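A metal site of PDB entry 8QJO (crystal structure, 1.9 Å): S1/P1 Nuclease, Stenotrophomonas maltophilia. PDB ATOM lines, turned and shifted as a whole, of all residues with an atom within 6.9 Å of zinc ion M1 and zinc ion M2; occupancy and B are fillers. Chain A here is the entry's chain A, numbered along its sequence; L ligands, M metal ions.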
ATOM      1  N   TRP A   1      20.271   8.901  27.340  1.00  0.00           N
ATOM      2  CA  TRP A   1      20.953   9.872  28.216  1.00  0.00           C
ATOM      3  C   TRP A   1      21.360   9.201  29.537  1.00  0.00           C
ATOM      4  O   TRP A   1      20.732   8.221  29.912  1.00  0.00           O
ATOM      5  CB  TRP A   1      20.082  11.123  28.498  1.00  0.00           C
ATOM      6  CG  TRP A   1      19.453  11.725  27.290  1.00  0.00           C
ATOM      7  CD1 TRP A   1      18.162  11.584  26.872  1.00  0.00           C
ATOM      8  CD2 TRP A   1      20.106  12.532  26.289  1.00  0.00           C
ATOM      9  NE1 TRP A   1      17.974  12.231  25.682  1.00  0.00           N
ATOM     10  CE2 TRP A   1      19.147  12.853  25.309  1.00  0.00           C
ATOM     11  CE3 TRP A   1      21.399  13.043  26.158  1.00  0.00           C
ATOM     12  CZ2 TRP A   1      19.433  13.617  24.193  1.00  0.00           C
ATOM     13  CZ3 TRP A   1      21.691  13.821  25.057  1.00  0.00           C
ATOM     14  CH2 TRP A   1      20.725  14.098  24.084  1.00  0.00           C
ATOM     15  N   GLY A   2      22.324   9.794  30.203  1.00  0.00           N
ATOM     16  CA  GLY A   2      22.635   9.561  31.624  1.00  0.00           C
ATOM     17  C   GLY A   2      21.527  10.112  32.481  1.00  0.00           C
ATOM     18  O   GLY A   2      20.580  10.702  31.897  1.00  0.00           O
ATOM     19  N   ALA A   3      21.621   9.938  33.802  1.00  0.00           N
ATOM     20  CA  ALA A   3      20.540  10.236  34.764  1.00  0.00           C
ATOM     21  C   ALA A   3      20.152  11.729  34.645  1.00  0.00           C
ATOM     22  O   ALA A   3      18.936  12.011  34.623  1.00  0.00           O
ATOM     23  CB  ALA A   3      20.969   9.848  36.161  1.00  0.00           C
ATOM     24  N   GLY A   5      20.398  13.923  32.064  1.00  0.00           N
ATOM     25  CA  GLY A   5      19.661  14.164  30.811  1.00  0.00           C
ATOM     26  C   GLY A   5      18.203  13.752  30.954  1.00  0.00           C
ATOM     27  O   GLY A   5      17.344  14.518  30.547  1.00  0.00           O
ATOM     28  N   HIS A   6      17.946  12.588  31.544  1.00  0.00           N
ATOM     29  CA  HIS A   6      16.580  12.079  31.826  1.00  0.00           C
ATOM     30  C   HIS A   6      15.808  13.070  32.712  1.00  0.00           C
ATOM     31  O   HIS A   6      14.595  13.347  32.406  1.00  0.00           O
ATOM     32  CB  HIS A   6      16.638  10.632  32.354  1.00  0.00           C
ATOM     33  CG  HIS A   6      16.901   9.705  31.213  1.00  0.00           C
ATOM     34  ND1 HIS A   6      15.959   9.494  30.233  1.00  0.00           N
ATOM     35  CD2 HIS A   6      18.001   9.035  30.845  1.00  0.00           C
ATOM     36  CE1 HIS A   6      16.455   8.646  29.339  1.00  0.00           C
ATOM     37  NE2 HIS A   6      17.732   8.394  29.660  1.00  0.00           N
ATOM     38  N   PRO A  42      15.133   8.490  35.406  1.00  0.00           N
ATOM     39  CA  PRO A  42      16.167   7.470  35.209  1.00  0.00           C
ATOM     40  C   PRO A  42      15.795   6.014  35.564  1.00  0.00           C
ATOM     41  O   PRO A  42      16.583   5.109  35.271  1.00  0.00           O
ATOM     42  CB  PRO A  42      17.318   7.925  36.148  1.00  0.00           C
ATOM     43  CG  PRO A  42      16.965   9.352  36.474  1.00  0.00           C
ATOM     44  CD  PRO A  42      15.453   9.332  36.572  1.00  0.00           C
ATOM     45  N   ALA A  44      14.049   3.378  34.582  1.00  0.00           N
ATOM     46  CA  ALA A  44      14.148   2.258  33.607  1.00  0.00           C
ATOM     47  C   ALA A  44      15.593   1.781  33.448  1.00  0.00           C
ATOM     48  O   ALA A  44      15.782   0.581  33.194  1.00  0.00           O
ATOM     49  CB  ALA A  44      13.535   2.694  32.299  1.00  0.00           C
ATOM     50  N   ASP A  45      16.592   2.662  33.596  1.00  0.00           N
ATOM     51  CA  ASP A  45      18.041   2.297  33.503  1.00  0.00           C
ATOM     52  C   ASP A  45      18.464   1.536  34.767  1.00  0.00           C
ATOM     53  O   ASP A  45      19.270   0.615  34.629  1.00  0.00           O
ATOM     54  CB  ASP A  45      18.971   3.496  33.308  1.00  0.00           C
ATOM     55  CG  ASP A  45      18.892   4.126  31.936  1.00  0.00           C
ATOM     56  OD1 ASP A  45      18.448   3.418  30.964  1.00  0.00           O
ATOM     57  OD2 ASP A  45      19.268   5.318  31.849  1.00  0.00           O
ATOM     58  N   ARG A  48      16.894  -1.901  34.373  1.00  0.00           N
ATOM     59  CA  ARG A  48      17.765  -2.653  33.432  1.00  0.00           C
ATOM     60  C   ARG A  48      18.985  -3.220  34.177  1.00  0.00           C
ATOM     61  O   ARG A  48      19.350  -4.359  33.927  1.00  0.00           O
ATOM     62  CB  ARG A  48      18.270  -1.776  32.278  1.00  0.00           C
ATOM     63  CG  ARG A  48      19.051  -2.557  31.235  1.00  0.00           C
ATOM     64  CD  ARG A  48      19.643  -1.709  30.124  1.00  0.00           C
ATOM     65  NE  ARG A  48      20.388  -0.571  30.668  1.00  0.00           N
ATOM     66  CZ  ARG A  48      20.430   0.647  30.155  1.00  0.00           C
ATOM     67  NH1 ARG A  48      19.797   0.976  29.013  1.00  0.00           N
ATOM     68  NH2 ARG A  48      21.147   1.558  30.796  1.00  0.00           N
ATOM     69  N   ALA A  59      15.653  -4.298  28.124  1.00  0.00           N
ATOM     70  CA  ALA A  59      16.925  -3.646  27.739  1.00  0.00           C
ATOM     71  C   ALA A  59      16.817  -3.111  26.314  1.00  0.00           C
ATOM     72  O   ALA A  59      17.197  -1.954  26.091  1.00  0.00           O
ATOM     73  CB  ALA A  59      18.121  -4.577  27.848  1.00  0.00           C
ATOM     74  N   TRP A  61      14.291  -2.081  24.804  1.00  0.00           N
ATOM     75  CA  TRP A  61      13.270  -0.989  24.709  1.00  0.00           C
ATOM     76  C   TRP A  61      13.945   0.398  24.680  1.00  0.00           C
ATOM     77  O   TRP A  61      13.234   1.357  24.389  1.00  0.00           O
ATOM     78  CB  TRP A  61      12.253  -1.040  25.846  1.00  0.00           C
ATOM     79  CG  TRP A  61      11.485  -2.318  26.002  1.00  0.00           C
ATOM     80  CD1 TRP A  61      11.619  -3.498  25.328  1.00  0.00           C
ATOM     81  CD2 TRP A  61      10.447  -2.541  26.970  1.00  0.00           C
ATOM     82  NE1 TRP A  61      10.716  -4.413  25.788  1.00  0.00           N
ATOM     83  CE2 TRP A  61      10.003  -3.859  26.813  1.00  0.00           C
ATOM     84  CE3 TRP A  61       9.877  -1.745  27.977  1.00  0.00           C
ATOM     85  CZ2 TRP A  61       9.001  -4.402  27.605  1.00  0.00           C
ATOM     86  CZ3 TRP A  61       8.890  -2.280  28.762  1.00  0.00           C
ATOM     87  CH2 TRP A  61       8.458  -3.594  28.576  1.00  0.00           C
ATOM     88  N   HIS A  62      15.236   0.516  24.998  1.00  0.00           N
ATOM     89  CA  HIS A  62      15.921   1.843  25.131  1.00  0.00           C
ATOM     90  C   HIS A  62      16.376   2.375  23.785  1.00  0.00           C
ATOM     91  O   HIS A  62      16.693   3.581  23.696  1.00  0.00           O
ATOM     92  CB  HIS A  62      17.064   1.782  26.155  1.00  0.00           C
ATOM     93  CG  HIS A  62      16.570   1.491  27.548  1.00  0.00           C
ATOM     94  ND1 HIS A  62      16.740   2.345  28.598  1.00  0.00           N
ATOM     95  CD2 HIS A  62      15.888   0.429  28.030  1.00  0.00           C
ATOM     96  CE1 HIS A  62      16.205   1.815  29.673  1.00  0.00           C
ATOM     97  NE2 HIS A  62      15.674   0.633  29.359  1.00  0.00           N
ATOM     98  N   TYR A  63      16.402   1.548  22.743  1.00  0.00           N
ATOM     99  CA  TYR A  63      17.032   1.926  21.464  1.00  0.00           C
ATOM    100  C   TYR A  63      16.359   1.224  20.292  1.00  0.00           C
ATOM    101  O   TYR A  63      15.454   0.370  20.445  1.00  0.00           O
ATOM    102  CB  TYR A  63      18.548   1.659  21.533  1.00  0.00           C
ATOM    103  CG  TYR A  63      18.889   0.208  21.722  1.00  0.00           C
ATOM    104  CD1 TYR A  63      18.903  -0.669  20.644  1.00  0.00           C
ATOM    105  CD2 TYR A  63      19.147  -0.300  22.982  1.00  0.00           C
ATOM    106  CE1 TYR A  63      19.202  -2.014  20.808  1.00  0.00           C
ATOM    107  CE2 TYR A  63      19.436  -1.643  23.156  1.00  0.00           C
ATOM    108  CZ  TYR A  63      19.468  -2.501  22.064  1.00  0.00           C
ATOM    109  OH  TYR A  63      19.745  -3.822  22.254  1.00  0.00           O
ATOM    110  N   ILE A  85      12.551   0.657  21.066  1.00  0.00           N
ATOM    111  CA  ILE A  85      12.027   1.890  21.705  1.00  0.00           C
ATOM    112  C   ILE A  85      10.767   2.360  20.958  1.00  0.00           C
ATOM    113  O   ILE A  85       9.887   2.841  21.639  1.00  0.00           O
ATOM    114  CB  ILE A  85      13.103   2.961  21.802  1.00  0.00           C
ATOM    115  CG1 ILE A  85      12.645   4.079  22.760  1.00  0.00           C
ATOM    116  CG2 ILE A  85      13.477   3.481  20.423  1.00  0.00           C
ATOM    117  CD1 ILE A  85      13.802   4.931  23.262  1.00  0.00           C
ATOM    118  N   HIS A 115      11.086   8.033  30.481  1.00  0.00           N
ATOM    119  CA  HIS A 115      12.458   7.597  30.127  1.00  0.00           C
ATOM    120  C   HIS A 115      12.616   7.529  28.603  1.00  0.00           C
ATOM    121  O   HIS A 115      13.613   8.048  28.086  1.00  0.00           O
ATOM    122  CB  HIS A 115      12.752   6.220  30.722  1.00  0.00           C
ATOM    123  CG  HIS A 115      14.184   5.868  30.578  1.00  0.00           C
ATOM    124  ND1 HIS A 115      15.134   6.391  31.432  1.00  0.00           N
ATOM    125  CD2 HIS A 115      14.828   5.115  29.655  1.00  0.00           C
ATOM    126  CE1 HIS A 115      16.332   5.955  31.060  1.00  0.00           C
ATOM    127  NE2 HIS A 115      16.166   5.193  29.934  1.00  0.00           N
ATOM    128  N   LEU A 116      11.675   6.861  27.927  1.00  0.00           N
ATOM    129  CA  LEU A 116      11.791   6.481  26.503  1.00  0.00           C
ATOM    130  C   LEU A 116      11.580   7.705  25.620  1.00  0.00           C
ATOM    131  O   LEU A 116      12.200   7.734  24.571  1.00  0.00           O
ATOM    132  CB  LEU A 116      10.792   5.373  26.152  1.00  0.00           C
ATOM    133  CG  LEU A 116      11.075   4.044  26.822  1.00  0.00           C
ATOM    134  CD1 LEU A 116      10.096   2.964  26.397  1.00  0.00           C
ATOM    135  CD2 LEU A 116      12.498   3.625  26.553  1.00  0.00           C
ATOM    136  N   GLY A 118      12.769  10.571  26.454  1.00  0.00           N
ATOM    137  CA  GLY A 118      14.177  11.005  26.606  1.00  0.00           C
ATOM    138  C   GLY A 118      15.098  10.270  25.654  1.00  0.00           C
ATOM    139  O   GLY A 118      15.716  10.885  24.791  1.00  0.00           O
ATOM    140  N   ASP A 119      15.203   8.954  25.807  1.00  0.00           N
ATOM    141  CA  ASP A 119      16.110   8.101  25.017  1.00  0.00           C
ATOM    142  C   ASP A 119      15.827   8.221  23.524  1.00  0.00           C
ATOM    143  O   ASP A 119      16.773   8.212  22.781  1.00  0.00           O
ATOM    144  CB  ASP A 119      16.030   6.641  25.454  1.00  0.00           C
ATOM    145  CG  ASP A 119      16.956   6.309  26.637  1.00  0.00           C
ATOM    146  OD1 ASP A 119      17.707   7.207  27.079  1.00  0.00           O
ATOM    147  OD2 ASP A 119      16.909   5.161  27.086  1.00  0.00           O
ATOM    148  N   GLN A 122      17.861  10.838  21.918  1.00  0.00           N
ATOM    149  CA  GLN A 122      19.336  10.735  21.958  1.00  0.00           C
ATOM    150  C   GLN A 122      19.743  10.135  20.615  1.00  0.00           C
ATOM    151  O   GLN A 122      19.389   8.989  20.309  1.00  0.00           O
ATOM    152  CB  GLN A 122      19.768   9.945  23.194  1.00  0.00           C
ATOM    153  CG  GLN A 122      21.138  10.293  23.777  1.00  0.00           C
ATOM    154  CD  GLN A 122      22.286   9.757  22.961  1.00  0.00           C
ATOM    155  OE1 GLN A 122      22.459  10.124  21.809  1.00  0.00           O
ATOM    156  NE2 GLN A 122      23.080   8.853  23.550  1.00  0.00           N
ATOM    157  N   HIS A 125      20.851   6.492  20.272  1.00  0.00           N
ATOM    158  CA  HIS A 125      19.784   5.503  20.588  1.00  0.00           C
ATOM    159  C   HIS A 125      19.005   5.073  19.318  1.00  0.00           C
ATOM    160  O   HIS A 125      18.094   4.207  19.415  1.00  0.00           O
ATOM    161  CB  HIS A 125      18.920   6.056  21.701  1.00  0.00           C
ATOM    162  CG  HIS A 125      19.512   5.853  23.055  1.00  0.00           C
ATOM    163  ND1 HIS A 125      18.889   5.091  24.021  1.00  0.00           N
ATOM    164  CD2 HIS A 125      20.636   6.337  23.643  1.00  0.00           C
ATOM    165  CE1 HIS A 125      19.624   5.087  25.115  1.00  0.00           C
ATOM    166  NE2 HIS A 125      20.689   5.833  24.914  1.00  0.00           N
ATOM    167  N   HIS A 149      28.807   6.561  22.301  1.00  0.00           N
ATOM    168  CA  HIS A 149      27.479   6.461  22.971  1.00  0.00           C
ATOM    169  C   HIS A 149      27.514   7.263  24.274  1.00  0.00           C
ATOM    170  O   HIS A 149      26.637   8.114  24.468  1.00  0.00           O
ATOM    171  CB  HIS A 149      27.021   5.014  23.204  1.00  0.00           C
ATOM    172  CG  HIS A 149      25.588   4.960  23.636  1.00  0.00           C
ATOM    173  ND1 HIS A 149      24.561   4.749  22.731  1.00  0.00           N
ATOM    174  CD2 HIS A 149      25.015   5.140  24.846  1.00  0.00           C
ATOM    175  CE1 HIS A 149      23.410   4.739  23.383  1.00  0.00           C
ATOM    176  NE2 HIS A 149      23.647   5.039  24.672  1.00  0.00           N
ATOM    177  N   ASP A 153      25.356  10.391  25.686  1.00  0.00           N
ATOM    178  CA  ASP A 153      24.580  10.135  26.923  1.00  0.00           C
ATOM    179  C   ASP A 153      24.866  11.188  27.981  1.00  0.00           C
ATOM    180  O   ASP A 153      23.876  11.696  28.585  1.00  0.00           O
ATOM    181  CB  ASP A 153      24.797   8.729  27.501  1.00  0.00           C
ATOM    182  CG  ASP A 153      23.835   7.695  26.955  1.00  0.00           C
ATOM    183  OD1 ASP A 153      22.874   8.103  26.189  1.00  0.00           O
ATOM    184  OD2 ASP A 153      23.980   6.518  27.352  1.00  0.00           O
HETATM  185  P1  LIG L   1      20.364   4.798  28.662  1.00  0.00           P
HETATM  186  O1  LIG L   1      21.330   4.259  29.703  1.00  0.00           O
HETATM  187  O2  LIG L   1      21.136   5.580  27.655  1.00  0.00           O
HETATM  188  O3  LIG L   1      19.348   5.732  29.348  1.00  0.00           O
HETATM  189  O4  LIG L   1      19.626   3.682  28.010  1.00  0.00           O
HETATM  190  P1  LG2 L   2      24.689  -1.193  27.839  1.00  0.00           P
HETATM  191  O1  LG2 L   2      23.896  -0.733  29.036  1.00  0.00           O
HETATM  192  O2  LG2 L   2      26.199  -1.346  28.014  1.00  0.00           O
HETATM  193  O3  LG2 L   2      24.082  -2.462  27.175  1.00  0.00           O
HETATM  194  O4  LG2 L   2      24.544  -0.004  26.679  1.00  0.00           O
HETATM  195  C1  LG2 L   2      24.926   1.342  26.964  1.00  0.00           C
HETATM  196  C2  LG2 L   2      23.967   2.246  26.242  1.00  0.00           C
HETATM  197  O5  LG2 L   2      23.921   1.865  24.854  1.00  0.00           O
HETATM  198  C3  LG2 L   2      22.518   2.255  26.743  1.00  0.00           C
HETATM  199  O6  LG2 L   2      21.997   3.582  26.739  1.00  0.00           O
HETATM  200  C4  LG2 L   2      21.819   1.273  25.789  1.00  0.00           C
HETATM  201  O7  LG2 L   2      20.456   1.603  25.545  1.00  0.00           O
HETATM  202  C5  LG2 L   2      22.599   1.491  24.488  1.00  0.00           C
HETATM  203  N1  LG2 L   2      22.703   0.327  23.605  1.00  0.00           N
HETATM  204  C6  LG2 L   2      23.074  -0.981  23.872  1.00  0.00           C
HETATM  205  N2  LG2 L   2      23.187  -1.725  22.781  1.00  0.00           N
HETATM  206  C7  LG2 L   2      22.821  -0.863  21.752  1.00  0.00           C
HETATM  207  C8  LG2 L   2      22.596  -1.105  20.376  1.00  0.00           C
HETATM  208  O8  LG2 L   2      22.686  -2.187  19.800  1.00  0.00           O
HETATM  209  N3  LG2 L   2      22.115   0.009  19.715  1.00  0.00           N
HETATM  210  C9  LG2 L   2      21.885   1.249  20.302  1.00  0.00           C
HETATM  211  N4  LG2 L   2      21.419   2.224  19.496  1.00  0.00           N
HETATM  212  N5  LG2 L   2      22.087   1.492  21.602  1.00  0.00           N
HETATM  213  C10 LG2 L   2      22.540   0.416  22.251  1.00  0.00           C
HETATM  214 ZN    ZN M   1      19.151   7.505  28.609  1.00  0.00          ZN
HETATM  215 ZN    ZN M   2      17.627   4.254  28.810  1.00  0.00          ZN
HETATM  216 ZN    ZN M   3      22.311   5.640  26.096  1.00  0.00          ZN
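NE of Arg 48 is in salt-bridge range of O1 of LG2 L2.
O of His 62 is in hydrogen-bond range of ND1 of His 125 (2.7 Å).
NE1 of Trp 1 is in hydrogen-bond range of O of Gly 118, at 2.8 Å.
A ring nitrogen (ND1) of His 6 sits close to a ring nitrogen (ND1) of His 115, at 3.4 Å.
ND1 of His 62 lies close to NH1 of Arg 48, 3.4 Å away.
The guanidinium group of Arg 48 sits close to the side-chain carboxylate of Asp 45 (3.3 Å).
Along chain A the residues within 4 Å of zinc ion M1 span positions 1 to 119.
The nearest printed residue that does not touch zinc ion M1 is His 115 (4.001 Å).
Residues that only touch zinc ion M2: Arg 48 (3.9 Å).
Within 4 Å of zinc ion M2: Asp 45, Arg 48, His 62, His 115 and Asp 119.
The nearest printed residue that does not touch zinc ion M2 is His 6 (4.2 Å).
Zinc ion M1 is bound by an oxygen (O3) of LIG L1, a ring nitrogen (NE2) of His 6, the side-chain carboxylate of Asp 119, the backbone carbonyl oxygen of Trp 1 and the backbone nitrogen of Trp 1.
Zinc ion M2 is bound by NE2 of His 115 (2.1 Å), OD2 of Asp 119 (2.1 Å), ND1 of His 62 (2.1 Å), O4 of LIG L1 (2.2 Å), O3 of LIG L1 (2.3 Å) and OD1 of Asp 45 (2.5 Å).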
